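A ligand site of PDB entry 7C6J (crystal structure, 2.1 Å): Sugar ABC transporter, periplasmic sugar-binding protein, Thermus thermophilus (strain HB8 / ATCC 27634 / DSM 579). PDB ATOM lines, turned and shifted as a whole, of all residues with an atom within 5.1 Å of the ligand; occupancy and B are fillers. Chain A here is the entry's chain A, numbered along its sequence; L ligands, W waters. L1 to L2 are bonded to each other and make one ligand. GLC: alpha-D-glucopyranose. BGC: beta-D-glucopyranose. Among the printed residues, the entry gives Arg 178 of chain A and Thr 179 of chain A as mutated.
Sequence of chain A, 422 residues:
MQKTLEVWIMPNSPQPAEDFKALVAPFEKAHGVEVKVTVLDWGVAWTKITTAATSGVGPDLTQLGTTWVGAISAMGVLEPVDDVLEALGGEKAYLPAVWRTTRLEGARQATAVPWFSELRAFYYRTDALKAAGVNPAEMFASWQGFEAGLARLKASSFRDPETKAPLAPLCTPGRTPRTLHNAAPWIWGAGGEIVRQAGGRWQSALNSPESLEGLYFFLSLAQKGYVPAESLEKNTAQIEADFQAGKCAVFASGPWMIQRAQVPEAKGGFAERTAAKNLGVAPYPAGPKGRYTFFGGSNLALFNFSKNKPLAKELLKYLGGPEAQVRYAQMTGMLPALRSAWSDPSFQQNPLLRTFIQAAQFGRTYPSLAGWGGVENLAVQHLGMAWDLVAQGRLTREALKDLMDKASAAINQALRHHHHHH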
ATOM      1  N   ASN A  12     -13.479  16.363   7.210  1.00  0.00           N
ATOM      2  CA  ASN A  12     -14.434  15.312   6.800  1.00  0.00           C
ATOM      3  C   ASN A  12     -13.690  14.203   6.024  1.00  0.00           C
ATOM      4  O   ASN A  12     -14.259  13.109   5.890  1.00  0.00           O
ATOM      5  CB  ASN A  12     -15.561  15.897   5.984  1.00  0.00           C
ATOM      6  CG  ASN A  12     -16.223  17.087   6.645  1.00  0.00           C
ATOM      7  OD1 ASN A  12     -16.639  16.998   7.816  1.00  0.00           O
ATOM      8  ND2 ASN A  12     -16.424  18.140   5.861  1.00  0.00           N
ATOM      9  N   TRP A  42     -13.186  19.625  14.941  1.00  0.00           N
ATOM     10  CA  TRP A  42     -14.513  19.554  15.582  1.00  0.00           C
ATOM     11  C   TRP A  42     -14.412  20.107  17.015  1.00  0.00           C
ATOM     12  O   TRP A  42     -15.355  20.798  17.448  1.00  0.00           O
ATOM     13  CB  TRP A  42     -15.063  18.126  15.591  1.00  0.00           C
ATOM     14  CG  TRP A  42     -15.714  17.717  14.329  1.00  0.00           C
ATOM     15  CD1 TRP A  42     -15.224  16.920  13.342  1.00  0.00           C
ATOM     16  CD2 TRP A  42     -16.975  18.211  13.869  1.00  0.00           C
ATOM     17  NE1 TRP A  42     -16.172  16.769  12.359  1.00  0.00           N
ATOM     18  CE2 TRP A  42     -17.245  17.555  12.649  1.00  0.00           C
ATOM     19  CE3 TRP A  42     -17.971  18.984  14.475  1.00  0.00           C
ATOM     20  CZ2 TRP A  42     -18.399  17.802  11.931  1.00  0.00           C
ATOM     21  CZ3 TRP A  42     -19.118  19.235  13.750  1.00  0.00           C
ATOM     22  CH2 TRP A  42     -19.339  18.620  12.511  1.00  0.00           C
ATOM     23  N   GLY A  65     -22.699  20.909  12.031  1.00  0.00           N
ATOM     24  CA  GLY A  65     -23.231  19.588  12.412  1.00  0.00           C
ATOM     25  C   GLY A  65     -24.739  19.649  12.426  1.00  0.00           C
ATOM     26  O   GLY A  65     -25.270  20.689  12.831  1.00  0.00           O
ATOM     27  N   THR A  66     -25.418  18.580  12.056  1.00  0.00           N
ATOM     28  CA  THR A  66     -26.897  18.614  11.994  1.00  0.00           C
ATOM     29  C   THR A  66     -27.414  19.019  13.374  1.00  0.00           C
ATOM     30  O   THR A  66     -28.415  19.805  13.422  1.00  0.00           O
ATOM     31  CB  THR A  66     -27.496  17.293  11.471  1.00  0.00           C
ATOM     32  OG1 THR A  66     -26.901  16.233  12.206  1.00  0.00           O
ATOM     33  CG2 THR A  66     -27.233  17.078   9.989  1.00  0.00           C
ATOM     34  N   THR A  67     -26.783  18.562  14.447  1.00  0.00           N
ATOM     35  CA  THR A  67     -27.305  18.761  15.826  1.00  0.00           C
ATOM     36  C   THR A  67     -27.190  20.213  16.265  1.00  0.00           C
ATOM     37  O   THR A  67     -27.718  20.543  17.298  1.00  0.00           O
ATOM     38  CB  THR A  67     -26.647  17.814  16.830  1.00  0.00           C
ATOM     39  OG1 THR A  67     -25.265  18.171  16.915  1.00  0.00           O
ATOM     40  CG2 THR A  67     -26.874  16.365  16.421  1.00  0.00           C
ATOM     41  N   TRP A  68     -26.459  21.033  15.513  1.00  0.00           N
ATOM     42  CA  TRP A  68     -26.116  22.445  15.862  1.00  0.00           C
ATOM     43  C   TRP A  68     -27.044  23.402  15.098  1.00  0.00           C
ATOM     44  O   TRP A  68     -27.014  24.609  15.367  1.00  0.00           O
ATOM     45  CB  TRP A  68     -24.652  22.715  15.519  1.00  0.00           C
ATOM     46  CG  TRP A  68     -23.684  21.989  16.417  1.00  0.00           C
ATOM     47  CD1 TRP A  68     -23.974  21.178  17.483  1.00  0.00           C
ATOM     48  CD2 TRP A  68     -22.260  22.013  16.343  1.00  0.00           C
ATOM     49  NE1 TRP A  68     -22.835  20.716  18.083  1.00  0.00           N
ATOM     50  CE2 TRP A  68     -21.769  21.194  17.395  1.00  0.00           C
ATOM     51  CE3 TRP A  68     -21.357  22.590  15.453  1.00  0.00           C
ATOM     52  CZ2 TRP A  68     -20.412  21.000  17.623  1.00  0.00           C
ATOM     53  CZ3 TRP A  68     -20.012  22.438  15.709  1.00  0.00           C
ATOM     54  CH2 TRP A  68     -19.554  21.643  16.758  1.00  0.00           C
ATOM     55  N   PHE A 116     -23.869  16.224   3.890  1.00  0.00           N
ATOM     56  CA  PHE A 116     -23.731  14.740   3.964  1.00  0.00           C
ATOM     57  C   PHE A 116     -24.426  14.208   5.219  1.00  0.00           C
ATOM     58  O   PHE A 116     -24.667  14.913   6.197  1.00  0.00           O
ATOM     59  CB  PHE A 116     -22.260  14.343   3.877  1.00  0.00           C
ATOM     60  CG  PHE A 116     -21.390  14.894   4.979  1.00  0.00           C
ATOM     61  CD1 PHE A 116     -21.315  14.254   6.214  1.00  0.00           C
ATOM     62  CD2 PHE A 116     -20.604  16.015   4.798  1.00  0.00           C
ATOM     63  CE1 PHE A 116     -20.487  14.718   7.229  1.00  0.00           C
ATOM     64  CE2 PHE A 116     -19.765  16.467   5.787  1.00  0.00           C
ATOM     65  CZ  PHE A 116     -19.720  15.838   7.015  1.00  0.00           C
ATOM     66  N   GLU A 118     -24.271  10.789   8.029  1.00  0.00           N
ATOM     67  CA  GLU A 118     -23.494   9.666   8.619  1.00  0.00           C
ATOM     68  C   GLU A 118     -24.340   9.048   9.730  1.00  0.00           C
ATOM     69  O   GLU A 118     -25.257   9.721  10.281  1.00  0.00           O
ATOM     70  CB  GLU A 118     -22.138  10.206   9.047  1.00  0.00           C
ATOM     71  CG  GLU A 118     -22.197  11.230  10.178  1.00  0.00           C
ATOM     72  CD  GLU A 118     -22.101  10.677  11.599  1.00  0.00           C
ATOM     73  OE1 GLU A 118     -21.996  11.515  12.486  1.00  0.00           O
ATOM     74  OE2 GLU A 118     -22.079   9.410  11.788  1.00  0.00           O
ATOM     75  N   ARG A 120     -24.137   5.486  12.771  1.00  0.00           N
ATOM     76  CA  ARG A 120     -23.156   4.718  13.555  1.00  0.00           C
ATOM     77  C   ARG A 120     -23.533   3.246  13.451  1.00  0.00           C
ATOM     78  O   ARG A 120     -24.736   2.897  13.463  1.00  0.00           O
ATOM     79  CB  ARG A 120     -23.115   5.230  14.999  1.00  0.00           C
ATOM     80  CG  ARG A 120     -22.786   6.711  15.093  1.00  0.00           C
ATOM     81  CD  ARG A 120     -21.570   7.087  14.356  1.00  0.00           C
ATOM     82  NE  ARG A 120     -21.397   8.528  14.281  1.00  0.00           N
ATOM     83  CZ  ARG A 120     -20.861   9.330  15.182  1.00  0.00           C
ATOM     84  NH1 ARG A 120     -20.364   8.919  16.347  1.00  0.00           N
ATOM     85  NH2 ARG A 120     -20.844  10.609  14.918  1.00  0.00           N
ATOM     86  N   ARG A 178     -17.035  14.357  24.087  1.00  0.00           N
ATOM     87  CA  ARG A 178     -17.540  15.578  23.392  1.00  0.00           C
ATOM     88  C   ARG A 178     -19.045  15.420  23.067  1.00  0.00           C
ATOM     89  O   ARG A 178     -19.753  16.476  22.991  1.00  0.00           O
ATOM     90  CB  ARG A 178     -16.738  15.861  22.113  1.00  0.00           C
ATOM     91  CG  ARG A 178     -16.206  17.288  22.028  1.00  0.00           C
ATOM     92  CD  ARG A 178     -16.104  17.922  20.615  1.00  0.00           C
ATOM     93  NE  ARG A 178     -15.175  17.159  19.775  1.00  0.00           N
ATOM     94  CZ  ARG A 178     -15.488  16.373  18.753  1.00  0.00           C
ATOM     95  NH1 ARG A 178     -16.749  16.240  18.315  1.00  0.00           N
ATOM     96  NH2 ARG A 178     -14.487  15.715  18.171  1.00  0.00           N
ATOM     97  N   THR A 179     -19.541  14.203  22.873  1.00  0.00           N
ATOM     98  CA  THR A 179     -20.957  13.986  22.421  1.00  0.00           C
ATOM     99  C   THR A 179     -21.649  12.852  23.199  1.00  0.00           C
ATOM    100  O   THR A 179     -21.016  11.997  23.802  1.00  0.00           O
ATOM    101  CB  THR A 179     -20.937  13.806  20.895  1.00  0.00           C
ATOM    102  OG1 THR A 179     -20.278  12.573  20.649  1.00  0.00           O
ATOM    103  CG2 THR A 179     -20.242  14.946  20.167  1.00  0.00           C
ATOM    104  N   HIS A 181     -23.200  10.806  21.268  1.00  0.00           N
ATOM    105  CA  HIS A 181     -23.518   9.925  20.115  1.00  0.00           C
ATOM    106  C   HIS A 181     -23.208   8.455  20.445  1.00  0.00           C
ATOM    107  O   HIS A 181     -23.912   7.564  19.915  1.00  0.00           O
ATOM    108  CB  HIS A 181     -22.766  10.299  18.825  1.00  0.00           C
ATOM    109  CG  HIS A 181     -22.815  11.717  18.444  1.00  0.00           C
ATOM    110  ND1 HIS A 181     -23.816  12.569  18.881  1.00  0.00           N
ATOM    111  CD2 HIS A 181     -21.938  12.499  17.791  1.00  0.00           C
ATOM    112  CE1 HIS A 181     -23.593  13.781  18.433  1.00  0.00           C
ATOM    113  NE2 HIS A 181     -22.465  13.783  17.775  1.00  0.00           N
ATOM    114  N   THR A 236     -12.118  10.035  20.717  1.00  0.00           N
ATOM    115  CA  THR A 236     -12.614   9.367  19.515  1.00  0.00           C
ATOM    116  C   THR A 236     -11.469   9.113  18.540  1.00  0.00           C
ATOM    117  O   THR A 236     -11.361   7.971  18.037  1.00  0.00           O
ATOM    118  CB  THR A 236     -13.685  10.245  18.841  1.00  0.00           C
ATOM    119  OG1 THR A 236     -14.789  10.226  19.748  1.00  0.00           O
ATOM    120  CG2 THR A 236     -14.074   9.713  17.489  1.00  0.00           C
ATOM    121  N   GLU A 240     -10.114   5.390  17.255  1.00  0.00           N
ATOM    122  CA  GLU A 240      -9.952   5.024  15.831  1.00  0.00           C
ATOM    123  C   GLU A 240      -8.536   4.494  15.603  1.00  0.00           C
ATOM    124  O   GLU A 240      -8.396   3.432  14.954  1.00  0.00           O
ATOM    125  CB  GLU A 240     -10.320   6.150  14.857  1.00  0.00           C
ATOM    126  CG  GLU A 240     -11.789   6.525  14.875  1.00  0.00           C
ATOM    127  CD  GLU A 240     -12.122   7.755  14.021  1.00  0.00           C
ATOM    128  OE1 GLU A 240     -11.157   8.315  13.431  1.00  0.00           O
ATOM    129  OE2 GLU A 240     -13.339   8.168  13.941  1.00  0.00           O
ATOM    130  N   TRP A 256     -17.108   6.702   7.416  1.00  0.00           N
ATOM    131  CA  TRP A 256     -15.818   7.262   6.952  1.00  0.00           C
ATOM    132  C   TRP A 256     -14.693   6.245   7.128  1.00  0.00           C
ATOM    133  O   TRP A 256     -13.723   6.299   6.322  1.00  0.00           O
ATOM    134  CB  TRP A 256     -15.486   8.570   7.646  1.00  0.00           C
ATOM    135  CG  TRP A 256     -15.424   8.484   9.133  1.00  0.00           C
ATOM    136  CD1 TRP A 256     -14.334   8.191   9.898  1.00  0.00           C
ATOM    137  CD2 TRP A 256     -16.482   8.812  10.038  1.00  0.00           C
ATOM    138  NE1 TRP A 256     -14.657   8.248  11.222  1.00  0.00           N
ATOM    139  CE2 TRP A 256     -15.976   8.661  11.342  1.00  0.00           C
ATOM    140  CE3 TRP A 256     -17.821   9.209   9.880  1.00  0.00           C
ATOM    141  CZ2 TRP A 256     -16.776   8.844  12.467  1.00  0.00           C
ATOM    142  CZ3 TRP A 256     -18.594   9.456  10.992  1.00  0.00           C
ATOM    143  CH2 TRP A 256     -18.080   9.287  12.263  1.00  0.00           C
ATOM    144  N   PHE A 294     -27.450   6.277  16.212  1.00  0.00           N
ATOM    145  CA  PHE A 294     -27.306   7.738  15.990  1.00  0.00           C
ATOM    146  C   PHE A 294     -27.216   7.991  14.473  1.00  0.00           C
ATOM    147  O   PHE A 294     -26.378   7.339  13.788  1.00  0.00           O
ATOM    148  CB  PHE A 294     -26.085   8.311  16.679  1.00  0.00           C
ATOM    149  CG  PHE A 294     -25.879   9.771  16.367  1.00  0.00           C
ATOM    150  CD1 PHE A 294     -26.674  10.734  16.955  1.00  0.00           C
ATOM    151  CD2 PHE A 294     -24.901  10.181  15.485  1.00  0.00           C
ATOM    152  CE1 PHE A 294     -26.530  12.075  16.638  1.00  0.00           C
ATOM    153  CE2 PHE A 294     -24.750  11.526  15.161  1.00  0.00           C
ATOM    154  CZ  PHE A 294     -25.567  12.471  15.719  1.00  0.00           C
ATOM    155  N   GLY A 296     -26.688  11.275  11.961  1.00  0.00           N
ATOM    156  CA  GLY A 296     -26.337  12.725  11.911  1.00  0.00           C
ATOM    157  C   GLY A 296     -25.717  13.092  10.597  1.00  0.00           C
ATOM    158  O   GLY A 296     -26.232  12.653   9.564  1.00  0.00           O
ATOM    159  N   GLY A 297     -24.634  13.876  10.640  1.00  0.00           N
ATOM    160  CA  GLY A 297     -24.072  14.432   9.406  1.00  0.00           C
ATOM    161  C   GLY A 297     -23.971  15.932   9.534  1.00  0.00           C
ATOM    162  O   GLY A 297     -24.044  16.444  10.679  1.00  0.00           O
ATOM    163  N   SER A 298     -23.685  16.596   8.428  1.00  0.00           N
ATOM    164  CA  SER A 298     -23.438  18.039   8.440  1.00  0.00           C
ATOM    165  C   SER A 298     -24.257  18.688   7.327  1.00  0.00           C
ATOM    166  O   SER A 298     -24.466  18.069   6.244  1.00  0.00           O
ATOM    167  CB  SER A 298     -21.930  18.343   8.318  1.00  0.00           C
ATOM    168  OG  SER A 298     -21.331  18.077   9.571  1.00  0.00           O
ATOM    169  N   MET A 334     -18.589   9.425   3.780  1.00  0.00           N
ATOM    170  CA  MET A 334     -19.926   9.749   4.306  1.00  0.00           C
ATOM    171  C   MET A 334     -20.978   9.281   3.287  1.00  0.00           C
ATOM    172  O   MET A 334     -20.641   8.863   2.204  1.00  0.00           O
ATOM    173  CB  MET A 334     -20.040  11.254   4.547  1.00  0.00           C
ATOM    174  CG  MET A 334     -18.929  11.785   5.420  1.00  0.00           C
ATOM    175  SD  MET A 334     -19.037  11.265   7.126  1.00  0.00           S
ATOM    176  CE  MET A 334     -17.550  12.074   7.750  1.00  0.00           C
ATOM    177  N   GLU A 376     -26.254  19.158  25.214  1.00  0.00           N
ATOM    178  CA  GLU A 376     -25.204  18.164  24.891  1.00  0.00           C
ATOM    179  C   GLU A 376     -24.000  18.408  25.795  1.00  0.00           C
ATOM    180  O   GLU A 376     -23.488  17.424  26.406  1.00  0.00           O
ATOM    181  CB  GLU A 376     -24.849  18.258  23.415  1.00  0.00           C
ATOM    182  CG  GLU A 376     -23.976  17.112  22.990  1.00  0.00           C
ATOM    183  CD  GLU A 376     -24.455  16.428  21.736  1.00  0.00           C
ATOM    184  OE1 GLU A 376     -24.835  17.152  20.765  1.00  0.00           O
ATOM    185  OE2 GLU A 376     -24.423  15.163  21.745  1.00  0.00           O
HETATM  186  C1  GLC L   1     -15.901  13.218  14.039  1.00  0.00           C
HETATM  187  C2  GLC L   1     -16.437  14.101  15.149  1.00  0.00           C
HETATM  188  C3  GLC L   1     -17.942  13.997  15.296  1.00  0.00           C
HETATM  189  C4  GLC L   1     -18.655  14.067  13.932  1.00  0.00           C
HETATM  190  C5  GLC L   1     -18.094  13.025  12.993  1.00  0.00           C
HETATM  191  C6  GLC L   1     -18.736  13.124  11.593  1.00  0.00           C
HETATM  192  O1  GLC L   1     -15.977  11.877  14.449  1.00  0.00           O
HETATM  193  O2  GLC L   1     -15.828  13.796  16.389  1.00  0.00           O
HETATM  194  O3  GLC L   1     -18.351  15.150  16.010  1.00  0.00           O
HETATM  195  O4  GLC L   1     -20.057  13.848  14.037  1.00  0.00           O
HETATM  196  O5  GLC L   1     -16.723  13.316  12.883  1.00  0.00           O
HETATM  197  O6  GLC L   1     -18.660  14.437  11.020  1.00  0.00           O
HETATM  198  C2  BGC L   2     -22.352  14.506  13.633  1.00  0.00           C
HETATM  199  C3  BGC L   2     -23.266  15.708  13.683  1.00  0.00           C
HETATM  200  C4  BGC L   2     -23.154  16.524  14.977  1.00  0.00           C
HETATM  201  C5  BGC L   2     -21.688  16.845  15.179  1.00  0.00           C
HETATM  202  C6  BGC L   2     -21.387  17.651  16.408  1.00  0.00           C
HETATM  203  C1  BGC L   2     -20.920  14.960  13.981  1.00  0.00           C
HETATM  204  O2  BGC L   2     -22.385  13.882  12.342  1.00  0.00           O
HETATM  205  O3  BGC L   2     -24.633  15.318  13.460  1.00  0.00           O
HETATM  206  O4  BGC L   2     -23.918  17.758  14.903  1.00  0.00           O
HETATM  207  O5  BGC L   2     -20.939  15.637  15.238  1.00  0.00           O
HETATM  208  O6  BGC L   2     -21.824  17.038  17.623  1.00  0.00           O
HETATM  209  O   HOH W   1     -18.943  17.633  18.603  1.00  0.00           O
HETATM  210  O   HOH W   2     -21.040  15.620  10.340  1.00  0.00           O
HETATM  211  O   HOH W   3     -17.344   9.836  15.910  1.00  0.00           O
HETATM  212  O   HOH W   4     -13.811  10.664  13.452  1.00  0.00           O
HETATM  213  O   HOH W   5     -16.439  15.239   9.979  1.00  0.00           O
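The side-chain carboxylate (OE1) of Glu 118 is in hydrogen-bond range of an oxygen (O2) of BGC L2 (2.4 Å).
The side-chain hydroxyl (OG1) of Thr 66 lies within hydrogen-bond range of an oxygen (O3) of BGC L2 (2.7 Å).
The backbone NH of Thr 67 is in hydrogen-bond range of an oxygen (O4) of BGC L2 (3.0 Å).
The guanidinium group (NH2) of Arg 178 lies within hydrogen-bond range of an oxygen (O2) of GLC L1, 2.9 Å away.
An oxygen (O4) of GLC L1 lies within hydrogen-bond range of the guanidinium group (NH2) of Arg 120, 3.4 Å away.
The backbone NH (N) of Gly 297 is in hydrogen-bond range of an oxygen (O2) of BGC L2.
The backbone carbonyl oxygen of Gly 297 sits at hydrogen-bond distance from an oxygen (O3) of BGC L2, 3.1 Å away.
The backbone NH of Thr 66 lies within hydrogen-bond range of an oxygen (O4) of BGC L2.
The side-chain hydroxyl (OG1) of Thr 67 sits at hydrogen-bond distance from an oxygen (O4) of BGC L2, at 2.5 Å.
O6 of BGC L2 is in hydrogen-bond range of NE2 of His 181 (3.3 Å).
The backbone NH (N) of His 181 lies close to the side-chain hydroxyl (OG1) of Thr 179.
The indole nitrogen (NE1) of Trp 256 sits at hydrogen-bond distance from the side-chain carboxylate (OE2) of Glu 240, 3.0 Å away.
The backbone carbonyl oxygen (O) of Glu 118 sits at hydrogen-bond distance from the backbone NH (N) of Gly 296, at 2.7 Å.
O of Phe 294 sits at hydrogen-bond distance from N of Arg 120, at 3.1 Å.
The backbone NH (N) of Thr 66 lies within hydrogen-bond range of the backbone carbonyl oxygen (O) of Gly 297, 2.9 Å away.
The guanidinium group (NE) of Arg 120 lies within salt-bridge range of the side-chain carboxylate (OE2) of Glu 118, at 2.7 Å.
CZ2 of Trp 42 touches O6 of GLC L1 (3.5 Å).
Gly 65 touches the ligand.
CZ2 of Trp 68 touches C6 of BGC L2, 3.7 Å away.
Thr 179 touches the ligand.
CZ2 of Trp 256 touches O1 of GLC L1, 3.7 Å away.
CZ of Phe 294 touches O3 of BGC L2 (3.8 Å).
Gly 296 touches the ligand.
Hydrophobic or aromatic side chains that line the ligand: Trp 42, Trp 68, His 181, Trp 256 and Phe 294.
Within 4 Å of the ligand: Trp 42, Gly 65, Thr 66, Thr 67, Trp 68, Glu 118, Arg 120, Arg 178, Thr 179, His 181, Trp 256, Phe 294, Gly 296 and Gly 297.
Water W5 lies within hydrogen-bond range of O6 of GLC L1, OD1 of Asn 12 and NE1 of Trp 42.
Water W4 lies within hydrogen-bond range of the side-chain carboxylate of Glu 240, an oxygen (O1) of GLC L1 and the indole nitrogen of Trp 256.
Water W2 lies within hydrogen-bond range of OG of Ser 298, O6 of GLC L1 and O of Gly 297.
Water W3 lies within hydrogen-bond range of an oxygen (O1) of GLC L1 and the guanidinium group (NH1) of Arg 120.
Water W1 bridges the guanidinium group of Arg 178 (2.6 Å) and an oxygen (O6) of BGC L2 (3.1 Å).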
